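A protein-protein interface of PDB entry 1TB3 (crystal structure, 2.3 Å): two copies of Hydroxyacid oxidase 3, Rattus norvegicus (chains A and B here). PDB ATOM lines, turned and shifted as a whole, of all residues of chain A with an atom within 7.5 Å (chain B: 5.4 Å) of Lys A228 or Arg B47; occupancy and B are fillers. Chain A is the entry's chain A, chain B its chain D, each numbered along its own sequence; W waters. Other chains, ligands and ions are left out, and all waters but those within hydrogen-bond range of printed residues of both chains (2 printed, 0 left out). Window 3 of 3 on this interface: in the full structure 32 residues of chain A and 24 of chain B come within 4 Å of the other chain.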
ATOM      1  N   ILE A 225     -23.599   5.229  -9.603  1.00  0.00           N
ATOM      2  CA  ILE A 225     -22.843   4.047 -10.002  1.00  0.00           C
ATOM      3  C   ILE A 225     -21.346   4.250  -9.741  1.00  0.00           C
ATOM      4  O   ILE A 225     -20.771   5.259 -10.142  1.00  0.00           O
ATOM      5  CB  ILE A 225     -23.102   3.719 -11.503  1.00  0.00           C
ATOM      6  CG1 ILE A 225     -24.538   3.208 -11.667  1.00  0.00           C
ATOM      7  CG2 ILE A 225     -22.105   2.684 -12.008  1.00  0.00           C
ATOM      8  CD1 ILE A 225     -24.896   2.839 -13.063  1.00  0.00           C
ATOM      9  N   LEU A 226     -20.729   3.289  -9.058  1.00  0.00           N
ATOM     10  CA  LEU A 226     -19.308   3.363  -8.724  1.00  0.00           C
ATOM     11  C   LEU A 226     -18.519   2.165  -9.235  1.00  0.00           C
ATOM     12  O   LEU A 226     -17.282   2.175  -9.202  1.00  0.00           O
ATOM     13  CB  LEU A 226     -19.123   3.451  -7.204  1.00  0.00           C
ATOM     14  CG  LEU A 226     -19.627   4.722  -6.517  1.00  0.00           C
ATOM     15  CD1 LEU A 226     -19.599   4.546  -5.012  1.00  0.00           C
ATOM     16  CD2 LEU A 226     -18.772   5.901  -6.947  1.00  0.00           C
ATOM     17  N   THR A 227     -19.224   1.140  -9.708  1.00  0.00           N
ATOM     18  CA  THR A 227     -18.564  -0.072 -10.189  1.00  0.00           C
ATOM     19  C   THR A 227     -18.873  -0.476 -11.625  1.00  0.00           C
ATOM     20  O   THR A 227     -19.908  -0.104 -12.180  1.00  0.00           O
ATOM     21  CB  THR A 227     -18.924  -1.265  -9.305  1.00  0.00           C
ATOM     22  OG1 THR A 227     -20.313  -1.586  -9.479  1.00  0.00           O
ATOM     23  CG2 THR A 227     -18.640  -0.940  -7.841  1.00  0.00           C
ATOM     24  N   LYS A 228     -17.972  -1.252 -12.222  1.00  0.00           N
ATOM     25  CA  LYS A 228     -18.185  -1.720 -13.584  1.00  0.00           C
ATOM     26  C   LYS A 228     -19.345  -2.712 -13.596  1.00  0.00           C
ATOM     27  O   LYS A 228     -20.080  -2.791 -14.578  1.00  0.00           O
ATOM     28  CB  LYS A 228     -16.919  -2.367 -14.158  1.00  0.00           C
ATOM     29  CG  LYS A 228     -16.384  -3.559 -13.381  1.00  0.00           C
ATOM     30  CD  LYS A 228     -15.071  -4.036 -14.001  1.00  0.00           C
ATOM     31  CE  LYS A 228     -14.551  -5.315 -13.355  1.00  0.00           C
ATOM     32  NZ  LYS A 228     -14.278  -5.169 -11.899  1.00  0.00           N
ATOM     33  N   GLU A 229     -19.522  -3.447 -12.497  1.00  0.00           N
ATOM     34  CA  GLU A 229     -20.617  -4.410 -12.419  1.00  0.00           C
ATOM     35  C   GLU A 229     -21.958  -3.708 -12.579  1.00  0.00           C
ATOM     36  O   GLU A 229     -22.796  -4.145 -13.369  1.00  0.00           O
ATOM     37  CB  GLU A 229     -20.596  -5.173 -11.090  1.00  0.00           C
ATOM     38  CG  GLU A 229     -19.425  -6.140 -10.915  1.00  0.00           C
ATOM     39  CD  GLU A 229     -18.126  -5.436 -10.583  1.00  0.00           C
ATOM     40  OE1 GLU A 229     -17.104  -6.124 -10.361  1.00  0.00           O
ATOM     41  OE2 GLU A 229     -18.127  -4.187 -10.539  1.00  0.00           O
ATOM     42  N   ASP A 230     -22.167  -2.626 -11.829  1.00  0.00           N
ATOM     43  CA  ASP A 230     -23.423  -1.881 -11.929  1.00  0.00           C
ATOM     44  C   ASP A 230     -23.512  -1.132 -13.257  1.00  0.00           C
ATOM     45  O   ASP A 230     -24.611  -0.879 -13.764  1.00  0.00           O
ATOM     46  CB  ASP A 230     -23.592  -0.905 -10.752  1.00  0.00           C
ATOM     47  CG  ASP A 230     -24.047  -1.601  -9.477  1.00  0.00           C
ATOM     48  OD1 ASP A 230     -24.172  -2.848  -9.477  1.00  0.00           O
ATOM     49  OD2 ASP A 230     -24.283  -0.907  -8.468  1.00  0.00           O
ATOM     50  N   ALA A 231     -22.365  -0.779 -13.832  1.00  0.00           N
ATOM     51  CA  ALA A 231     -22.387  -0.088 -15.121  1.00  0.00           C
ATOM     52  C   ALA A 231     -22.867  -1.076 -16.199  1.00  0.00           C
ATOM     53  O   ALA A 231     -23.576  -0.693 -17.131  1.00  0.00           O
ATOM     54  CB  ALA A 231     -21.002   0.451 -15.468  1.00  0.00           C
ATOM     55  N   GLU A 232     -22.477  -2.345 -16.069  1.00  0.00           N
ATOM     56  CA  GLU A 232     -22.906  -3.372 -17.020  1.00  0.00           C
ATOM     57  C   GLU A 232     -24.425  -3.544 -16.887  1.00  0.00           C
ATOM     58  O   GLU A 232     -25.150  -3.548 -17.885  1.00  0.00           O
ATOM     59  CB  GLU A 232     -22.219  -4.712 -16.732  1.00  0.00           C
ATOM     60  CG  GLU A 232     -20.714  -4.755 -16.998  1.00  0.00           C
ATOM     61  CD  GLU A 232     -20.352  -4.582 -18.472  1.00  0.00           C
ATOM     62  OE1 GLU A 232     -21.265  -4.619 -19.328  1.00  0.00           O
ATOM     63  OE2 GLU A 232     -19.149  -4.420 -18.774  1.00  0.00           O
ATOM     64  N   LEU A 233     -24.904  -3.681 -15.652  1.00  0.00           N
ATOM     65  CA  LEU A 233     -26.334  -3.838 -15.410  1.00  0.00           C
ATOM     66  C   LEU A 233     -27.107  -2.652 -15.956  1.00  0.00           C
ATOM     67  O   LEU A 233     -28.206  -2.813 -16.479  1.00  0.00           O
ATOM     68  CB  LEU A 233     -26.623  -3.985 -13.912  1.00  0.00           C
ATOM     69  CG  LEU A 233     -26.182  -5.302 -13.267  1.00  0.00           C
ATOM     70  CD1 LEU A 233     -26.508  -5.303 -11.778  1.00  0.00           C
ATOM     71  CD2 LEU A 233     -26.898  -6.451 -13.964  1.00  0.00           C
ATOM     72  N   ALA A 234     -26.535  -1.458 -15.838  1.00  0.00           N
ATOM     73  CA  ALA A 234     -27.202  -0.261 -16.326  1.00  0.00           C
ATOM     74  C   ALA A 234     -27.419  -0.373 -17.829  1.00  0.00           C
ATOM     75  O   ALA A 234     -28.475  -0.008 -18.341  1.00  0.00           O
ATOM     76  CB  ALA A 234     -26.373   0.979 -16.007  1.00  0.00           C
ATOM     77  N   MET A 235     -26.417  -0.878 -18.540  1.00  0.00           N
ATOM     78  CA  MET A 235     -26.530  -1.017 -19.983  1.00  0.00           C
ATOM     79  C   MET A 235     -27.516  -2.121 -20.354  1.00  0.00           C
ATOM     80  O   MET A 235     -28.308  -1.952 -21.274  1.00  0.00           O
ATOM     81  CB  MET A 235     -25.151  -1.267 -20.606  1.00  0.00           C
ATOM     82  CG  MET A 235     -24.226  -0.054 -20.487  1.00  0.00           C
ATOM     83  SD  MET A 235     -22.679  -0.196 -21.398  1.00  0.00           S
ATOM     84  CE  MET A 235     -21.761  -1.359 -20.390  1.00  0.00           C
ATOM     85  N   LEU A 252     -22.675   6.079   1.633  1.00  0.00           N
ATOM     86  CA  LEU A 252     -21.797   5.003   2.096  1.00  0.00           C
ATOM     87  C   LEU A 252     -20.396   5.611   2.085  1.00  0.00           C
ATOM     88  O   LEU A 252     -19.888   5.968   1.032  1.00  0.00           O
ATOM     89  CB  LEU A 252     -21.832   3.807   1.139  1.00  0.00           C
ATOM     90  CG  LEU A 252     -21.545   2.406   1.702  1.00  0.00           C
ATOM     91  CD1 LEU A 252     -20.836   1.586   0.653  1.00  0.00           C
ATOM     92  CD2 LEU A 252     -20.704   2.472   2.953  1.00  0.00           C
ATOM     93  N   GLU A 254     -16.154   5.799   2.712  1.00  0.00           N
ATOM     94  CA  GLU A 254     -14.994   4.968   2.458  1.00  0.00           C
ATOM     95  C   GLU A 254     -15.083   4.152   1.171  1.00  0.00           C
ATOM     96  O   GLU A 254     -14.538   3.055   1.070  1.00  0.00           O
ATOM     97  CB  GLU A 254     -14.702   4.086   3.686  1.00  0.00           C
ATOM     98  CG  GLU A 254     -14.700   4.908   4.975  1.00  0.00           C
ATOM     99  CD  GLU A 254     -14.073   4.207   6.163  1.00  0.00           C
ATOM    100  OE1 GLU A 254     -14.327   4.651   7.306  1.00  0.00           O
ATOM    101  OE2 GLU A 254     -13.319   3.230   5.968  1.00  0.00           O
ATOM    102  N   VAL A 255     -15.791   4.698   0.189  1.00  0.00           N
ATOM    103  CA  VAL A 255     -15.884   4.072  -1.124  1.00  0.00           C
ATOM    104  C   VAL A 255     -14.868   4.872  -1.950  1.00  0.00           C
ATOM    105  O   VAL A 255     -14.269   5.824  -1.437  1.00  0.00           O
ATOM    106  CB  VAL A 255     -17.288   4.224  -1.755  1.00  0.00           C
ATOM    107  CG1 VAL A 255     -18.328   3.530  -0.875  1.00  0.00           C
ATOM    108  CG2 VAL A 255     -17.627   5.707  -1.954  1.00  0.00           C
ATOM    109  N   SER A 256     -14.663   4.506  -3.212  1.00  0.00           N
ATOM    110  CA  SER A 256     -13.700   5.236  -4.028  1.00  0.00           C
ATOM    111  C   SER A 256     -14.128   6.661  -4.324  1.00  0.00           C
ATOM    112  O   SER A 256     -15.313   7.006  -4.290  1.00  0.00           O
ATOM    113  CB  SER A 256     -13.445   4.519  -5.360  1.00  0.00           C
ATOM    114  OG  SER A 256     -12.621   3.381  -5.165  1.00  0.00           O
ATOM    115  N   ALA A 261     -13.365   6.261  -9.508  1.00  0.00           N
ATOM    116  CA  ALA A 261     -14.348   5.268  -9.935  1.00  0.00           C
ATOM    117  C   ALA A 261     -14.737   5.470 -11.404  1.00  0.00           C
ATOM    118  O   ALA A 261     -15.116   4.520 -12.095  1.00  0.00           O
ATOM    119  CB  ALA A 261     -15.594   5.361  -9.049  1.00  0.00           C
ATOM    120  N   ARG A 263     -12.997   5.902 -13.957  1.00  0.00           N
ATOM    121  CA  ARG A 263     -12.196   5.111 -14.878  1.00  0.00           C
ATOM    122  C   ARG A 263     -12.776   3.748 -15.203  1.00  0.00           C
ATOM    123  O   ARG A 263     -12.969   3.439 -16.376  1.00  0.00           O
ATOM    124  CB  ARG A 263     -10.754   4.960 -14.363  1.00  0.00           C
ATOM    125  CG  ARG A 263     -10.051   6.292 -14.097  1.00  0.00           C
ATOM    126  CD  ARG A 263      -8.532   6.148 -14.023  1.00  0.00           C
ATOM    127  NE  ARG A 263      -7.898   7.345 -13.470  1.00  0.00           N
ATOM    128  CZ  ARG A 263      -6.638   7.710 -13.705  1.00  0.00           C
ATOM    129  NH1 ARG A 263      -5.865   6.973 -14.490  1.00  0.00           N
ATOM    130  NH2 ARG A 263      -6.147   8.813 -13.148  1.00  0.00           N
ATOM    131  N   GLU A 264     -13.080   2.941 -14.190  1.00  0.00           N
ATOM    132  CA  GLU A 264     -13.601   1.610 -14.469  1.00  0.00           C
ATOM    133  C   GLU A 264     -14.995   1.652 -15.075  1.00  0.00           C
ATOM    134  O   GLU A 264     -15.356   0.763 -15.840  1.00  0.00           O
ATOM    135  CB  GLU A 264     -13.565   0.723 -13.215  1.00  0.00           C
ATOM    136  CG  GLU A 264     -14.716   0.862 -12.242  1.00  0.00           C
ATOM    137  CD  GLU A 264     -14.629  -0.169 -11.126  1.00  0.00           C
ATOM    138  OE1 GLU A 264     -13.666  -0.106 -10.338  1.00  0.00           O
ATOM    139  OE2 GLU A 264     -15.511  -1.054 -11.036  1.00  0.00           O
ATOM    140  N   VAL A 265     -15.770   2.684 -14.752  1.00  0.00           N
ATOM    141  CA  VAL A 265     -17.107   2.819 -15.324  1.00  0.00           C
ATOM    142  C   VAL A 265     -16.997   3.173 -16.812  1.00  0.00           C
ATOM    143  O   VAL A 265     -17.698   2.604 -17.651  1.00  0.00           O
ATOM    144  CB  VAL A 265     -17.938   3.907 -14.607  1.00  0.00           C
ATOM    145  CG1 VAL A 265     -19.236   4.160 -15.369  1.00  0.00           C
ATOM    146  CG2 VAL A 265     -18.261   3.462 -13.192  1.00  0.00           C
ATOM    147  N   VAL A 266     -16.119   4.115 -17.138  1.00  0.00           N
ATOM    148  CA  VAL A 266     -15.926   4.518 -18.529  1.00  0.00           C
ATOM    149  C   VAL A 266     -15.405   3.338 -19.356  1.00  0.00           C
ATOM    150  O   VAL A 266     -15.838   3.119 -20.478  1.00  0.00           O
ATOM    151  CB  VAL A 266     -14.912   5.698 -18.647  1.00  0.00           C
ATOM    152  CG1 VAL A 266     -14.367   5.804 -20.081  1.00  0.00           C
ATOM    153  CG2 VAL A 266     -15.589   7.007 -18.262  1.00  0.00           C
ATOM    154  N   ALA A 267     -14.471   2.583 -18.792  1.00  0.00           N
ATOM    155  CA  ALA A 267     -13.904   1.443 -19.495  1.00  0.00           C
ATOM    156  C   ALA A 267     -14.950   0.363 -19.773  1.00  0.00           C
ATOM    157  O   ALA A 267     -14.905  -0.290 -20.813  1.00  0.00           O
ATOM    158  CB  ALA A 267     -12.745   0.853 -18.690  1.00  0.00           C
ATOM    159  N   ALA A 268     -15.890   0.180 -18.849  1.00  0.00           N
ATOM    160  CA  ALA A 268     -16.926  -0.833 -19.014  1.00  0.00           C
ATOM    161  C   ALA A 268     -17.977  -0.419 -20.039  1.00  0.00           C
ATOM    162  O   ALA A 268     -18.433  -1.237 -20.839  1.00  0.00           O
ATOM    163  CB  ALA A 268     -17.594  -1.122 -17.675  1.00  0.00           C
ATOM    164  N   VAL A 269     -18.354   0.854 -20.011  1.00  0.00           N
ATOM    165  CA  VAL A 269     -19.362   1.394 -20.919  1.00  0.00           C
ATOM    166  C   VAL A 269     -18.887   1.482 -22.367  1.00  0.00           C
ATOM    167  O   VAL A 269     -19.696   1.427 -23.293  1.00  0.00           O
ATOM    168  CB  VAL A 269     -19.837   2.789 -20.421  1.00  0.00           C
ATOM    169  CG1 VAL A 269     -20.692   3.478 -21.467  1.00  0.00           C
ATOM    170  CG2 VAL A 269     -20.633   2.615 -19.133  1.00  0.00           C
ATOM    171  N   ARG B  45     -10.973   0.498   0.499  1.00  0.00           N
ATOM    172  CA  ARG B  45     -12.077   1.063  -0.270  1.00  0.00           C
ATOM    173  C   ARG B  45     -13.182   0.030  -0.493  1.00  0.00           C
ATOM    174  O   ARG B  45     -12.907  -1.134  -0.736  1.00  0.00           O
ATOM    175  CB  ARG B  45     -11.554   1.604  -1.607  1.00  0.00           C
ATOM    176  CG  ARG B  45     -10.607   2.800  -1.448  1.00  0.00           C
ATOM    177  CD  ARG B  45     -11.372   4.070  -1.046  1.00  0.00           C
ATOM    178  NE  ARG B  45     -10.501   5.098  -0.476  1.00  0.00           N
ATOM    179  CZ  ARG B  45     -10.268   5.253   0.826  1.00  0.00           C
ATOM    180  NH1 ARG B  45     -10.852   4.453   1.717  1.00  0.00           N
ATOM    181  NH2 ARG B  45      -9.430   6.200   1.238  1.00  0.00           N
ATOM    182  N   LEU B  46     -14.429   0.474  -0.398  1.00  0.00           N
ATOM    183  CA  LEU B  46     -15.584  -0.387  -0.575  1.00  0.00           C
ATOM    184  C   LEU B  46     -16.159  -0.300  -1.984  1.00  0.00           C
ATOM    185  O   LEU B  46     -16.090   0.748  -2.623  1.00  0.00           O
ATOM    186  CB  LEU B  46     -16.667  -0.004   0.437  1.00  0.00           C
ATOM    187  CG  LEU B  46     -16.334  -0.255   1.911  1.00  0.00           C
ATOM    188  CD1 LEU B  46     -17.407   0.370   2.801  1.00  0.00           C
ATOM    189  CD2 LEU B  46     -16.220  -1.756   2.164  1.00  0.00           C
ATOM    190  N   ARG B  47     -16.727  -1.405  -2.458  1.00  0.00           N
ATOM    191  CA  ARG B  47     -17.337  -1.464  -3.786  1.00  0.00           C
ATOM    192  C   ARG B  47     -18.807  -1.825  -3.619  1.00  0.00           C
ATOM    193  O   ARG B  47     -19.162  -3.002  -3.608  1.00  0.00           O
ATOM    194  CB  ARG B  47     -16.660  -2.535  -4.637  1.00  0.00           C
ATOM    195  CG  ARG B  47     -15.211  -2.265  -4.928  1.00  0.00           C
ATOM    196  CD  ARG B  47     -14.592  -3.432  -5.670  1.00  0.00           C
ATOM    197  NE  ARG B  47     -15.237  -3.681  -6.956  1.00  0.00           N
ATOM    198  CZ  ARG B  47     -15.131  -2.877  -8.005  1.00  0.00           C
ATOM    199  NH1 ARG B  47     -14.405  -1.767  -7.924  1.00  0.00           N
ATOM    200  NH2 ARG B  47     -15.742  -3.187  -9.142  1.00  0.00           N
ATOM    201  N   PRO B  48     -19.685  -0.817  -3.505  1.00  0.00           N
ATOM    202  CA  PRO B  48     -21.112  -1.086  -3.329  1.00  0.00           C
ATOM    203  C   PRO B  48     -21.846  -1.565  -4.577  1.00  0.00           C
ATOM    204  O   PRO B  48     -21.475  -1.239  -5.698  1.00  0.00           O
ATOM    205  CB  PRO B  48     -21.646   0.253  -2.833  1.00  0.00           C
ATOM    206  CG  PRO B  48     -20.850   1.220  -3.642  1.00  0.00           C
ATOM    207  CD  PRO B  48     -19.429   0.634  -3.583  1.00  0.00           C
ATOM    208  N   ARG B  49     -22.898  -2.345  -4.357  1.00  0.00           N
ATOM    209  CA  ARG B  49     -23.735  -2.850  -5.433  1.00  0.00           C
ATOM    210  C   ARG B  49     -25.133  -2.332  -5.126  1.00  0.00           C
ATOM    211  O   ARG B  49     -25.753  -2.721  -4.134  1.00  0.00           O
ATOM    212  CB  ARG B  49     -23.703  -4.379  -5.457  1.00  0.00           C
ATOM    213  CG  ARG B  49     -22.304  -4.961  -5.709  1.00  0.00           C
ATOM    214  CD  ARG B  49     -21.666  -4.322  -6.955  1.00  0.00           C
ATOM    215  NE  ARG B  49     -22.532  -4.452  -8.126  1.00  0.00           N
ATOM    216  CZ  ARG B  49     -22.747  -5.592  -8.779  1.00  0.00           C
ATOM    217  NH1 ARG B  49     -22.156  -6.713  -8.385  1.00  0.00           N
ATOM    218  NH2 ARG B  49     -23.562  -5.613  -9.824  1.00  0.00           N
ATOM    219  N   SER B 334     -24.452  -0.910   0.875  1.00  0.00           N
ATOM    220  CA  SER B 334     -23.541  -1.667   0.018  1.00  0.00           C
ATOM    221  C   SER B 334     -24.196  -2.817  -0.745  1.00  0.00           C
ATOM    222  O   SER B 334     -23.603  -3.349  -1.682  1.00  0.00           O
ATOM    223  CB  SER B 334     -22.361  -2.203   0.837  1.00  0.00           C
ATOM    224  OG  SER B 334     -22.801  -3.157   1.786  1.00  0.00           O
ATOM    225  N   ASP B 345     -15.772  -9.331  -2.558  1.00  0.00           N
ATOM    226  CA  ASP B 345     -16.046  -8.595  -3.795  1.00  0.00           C
ATOM    227  C   ASP B 345     -16.310  -7.143  -3.409  1.00  0.00           C
ATOM    228  O   ASP B 345     -16.222  -6.223  -4.230  1.00  0.00           O
ATOM    229  CB  ASP B 345     -17.298  -9.133  -4.495  1.00  0.00           C
ATOM    230  CG  ASP B 345     -17.090 -10.497  -5.116  1.00  0.00           C
ATOM    231  OD1 ASP B 345     -18.078 -11.043  -5.651  1.00  0.00           O
ATOM    232  OD2 ASP B 345     -15.952 -11.018  -5.076  1.00  0.00           O
ATOM    233  N   LEU B 346     -16.642  -6.964  -2.139  1.00  0.00           N
ATOM    234  CA  LEU B 346     -16.956  -5.665  -1.563  1.00  0.00           C
ATOM    235  C   LEU B 346     -15.680  -4.844  -1.390  1.00  0.00           C
ATOM    236  O   LEU B 346     -15.716  -3.611  -1.390  1.00  0.00           O
ATOM    237  CB  LEU B 346     -17.621  -5.905  -0.216  1.00  0.00           C
ATOM    238  CG  LEU B 346     -18.740  -5.037   0.340  1.00  0.00           C
ATOM    239  CD1 LEU B 346     -19.829  -4.769  -0.692  1.00  0.00           C
ATOM    240  CD2 LEU B 346     -19.302  -5.781   1.544  1.00  0.00           C
ATOM    241  N   ILE B 347     -14.554  -5.546  -1.271  1.00  0.00           N
ATOM    242  CA  ILE B 347     -13.246  -4.930  -1.068  1.00  0.00           C
ATOM    243  C   ILE B 347     -12.476  -4.617  -2.345  1.00  0.00           C
ATOM    244  O   ILE B 347     -12.349  -5.458  -3.230  1.00  0.00           O
ATOM    245  CB  ILE B 347     -12.358  -5.838  -0.196  1.00  0.00           C
ATOM    246  CG1 ILE B 347     -13.035  -6.089   1.154  1.00  0.00           C
ATOM    247  CG2 ILE B 347     -10.992  -5.211  -0.020  1.00  0.00           C
ATOM    248  CD1 ILE B 347     -13.332  -4.820   1.929  1.00  0.00           C
ATOM    249  N   GLN B 348     -11.941  -3.405  -2.426  1.00  0.00           N
ATOM    250  CA  GLN B 348     -11.173  -2.986  -3.593  1.00  0.00           C
ATOM    251  C   GLN B 348      -9.750  -3.524  -3.471  1.00  0.00           C
ATOM    252  O   GLN B 348      -9.041  -3.207  -2.519  1.00  0.00           O
ATOM    253  CB  GLN B 348     -11.139  -1.458  -3.680  1.00  0.00           C
ATOM    254  CG  GLN B 348     -10.369  -0.904  -4.876  1.00  0.00           C
ATOM    255  CD  GLN B 348     -11.144  -0.991  -6.179  1.00  0.00           C
ATOM    256  OE1 GLN B 348     -12.228  -0.420  -6.312  1.00  0.00           O
ATOM    257  NE2 GLN B 348     -10.591  -1.704  -7.150  1.00  0.00           N
HETATM  258  O   HOH W   1     -16.104   2.501  -4.545  1.00  0.00           O
HETATM  259  O   HOH W   2     -21.859   0.690  -8.022  1.00  0.00           O
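The side-chain amide oxygen (OE1) of Gln B348 sits at hydrogen-bond distance from the guanidinium group (NH1) of Arg B47, at 3.0 Å.
N of Arg B49 sits at hydrogen-bond distance from O of Ser B334 (2.9 Å).
The side-chain carboxylate of Glu A229 is in salt-bridge range of the side-chain amino group of Lys A228 (3.4 Å).
The backbone carbonyl oxygen of Arg B45 sits at hydrogen-bond distance from the backbone NH of Gln B348.
The side-chain hydroxyl of Thr A227 sits at hydrogen-bond distance from the backbone NH of Asp A230, at 3.2 Å.
The backbone NH (N) of Arg B47 lies within hydrogen-bond range of the backbone carbonyl oxygen (O) of Leu B346 (2.7 Å).
OE2 of Glu A229 is in salt-bridge range of NH2 of Arg B47, at 2.9 Å.
The guanidinium group of Arg B49 is in salt-bridge range of the side-chain carboxylate of Asp A230, 2.7 Å away.
OE2 of Glu A264 lies within salt-bridge range of NH2 of Arg B47 (2.9 Å).
The backbone carbonyl oxygen of Glu A254 is in hydrogen-bond range of the backbone NH of Leu B46, at 3.0 Å.
Water W1 lies within hydrogen-bond range of the backbone carbonyl oxygen of Leu B46 (2.6 Å) and the backbone NH of Ser A256 (2.8 Å).
Water W2 lies within hydrogen-bond range of OD2 of Asp A230 (2.9 Å), N of Leu A226 (3.0 Å), O of Pro B48 (3.0 Å) and OG1 of Thr A227 (3.1 Å).
Among the printed residues, merely in contact across the chains: Leu A226 with Pro B48 (3.8 Å), Thr A227 with Arg B47 (3.7 Å), Thr A227 with Pro B48 (3.6 Å), Thr A227 with Arg B49 (3.9 Å), Lys A228 with Arg B47 (3.7 Å), Glu A229 with Arg B49 (3.2 Å), Asp A230 with Pro B48 (3.96 Å), Leu A233 with Arg B49 (3.5 Å), Leu A252 with Leu B46 (3.9 Å), Leu A252 with Pro B48 (3.8 Å), Glu A254 with Arg B45 (3.4 Å), Val A255 with Arg B45 (3.4 Å), Val A255 with Leu B46 (3.7 Å), Ser A256 with Arg B45 (3.96 Å) and Ser A256 with Gln B348 (3.99 Å).
Of the printed residues of chain B, Lys A228 touches Arg B47.
Of chain A, only Thr A227 (3.7 Å), Lys A228 (3.7 Å), Glu A229 (2.9 Å) and Glu A264 (2.9 Å) come within 4 Å of Arg B47.
Of the printed residues of chain B, Glu A254 touches Arg B45 (3.4 Å) and Leu B46 (3.0 Å).
Of the printed residues of chain B, Glu A264 touches Arg B47 (2.9 Å).
Printed residues of chain B within 4 Å of Asp A230: Pro B48 (3.96 Å) and Arg B49 (2.7 Å).
Of the printed residues of chain A, Pro B48 touches Leu A226, Thr A227, Asp A230 and Leu A252.
Of the printed residues of chain B, Leu A226 touches Pro B48.
Hydrophobic or aromatic side chains of chain B that line the printed part of chain A: Leu B46 and Pro B48.
Along chain B the printed residues that touch a printed residue of chain A span positions 45 to 348.
Of the 23 printed residues of chain A, 11 touch a printed residue of chain B.
Printed residues of chain A that touch a printed residue of chain B: Leu A226, Thr A227, Lys A228, Glu A229, Asp A230, Leu A233, Leu A252, Glu A254, Val A255, Ser A256 and Glu A264.
Among the printed residues, 19 pairs touch across the chains.
Among the printed residues, Asp or Glu carboxylates within 4 Å of a Lys or Arg side-chain nitrogen of the other chain: Glu A229 with Arg B47, Asp A230 with Arg B49 and Glu A264 with Arg B47.
No position is printed for both chains.
Of the 19 pairs that touch across the chains among the printed residues, none has its exchanged pair printed and touching as well.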
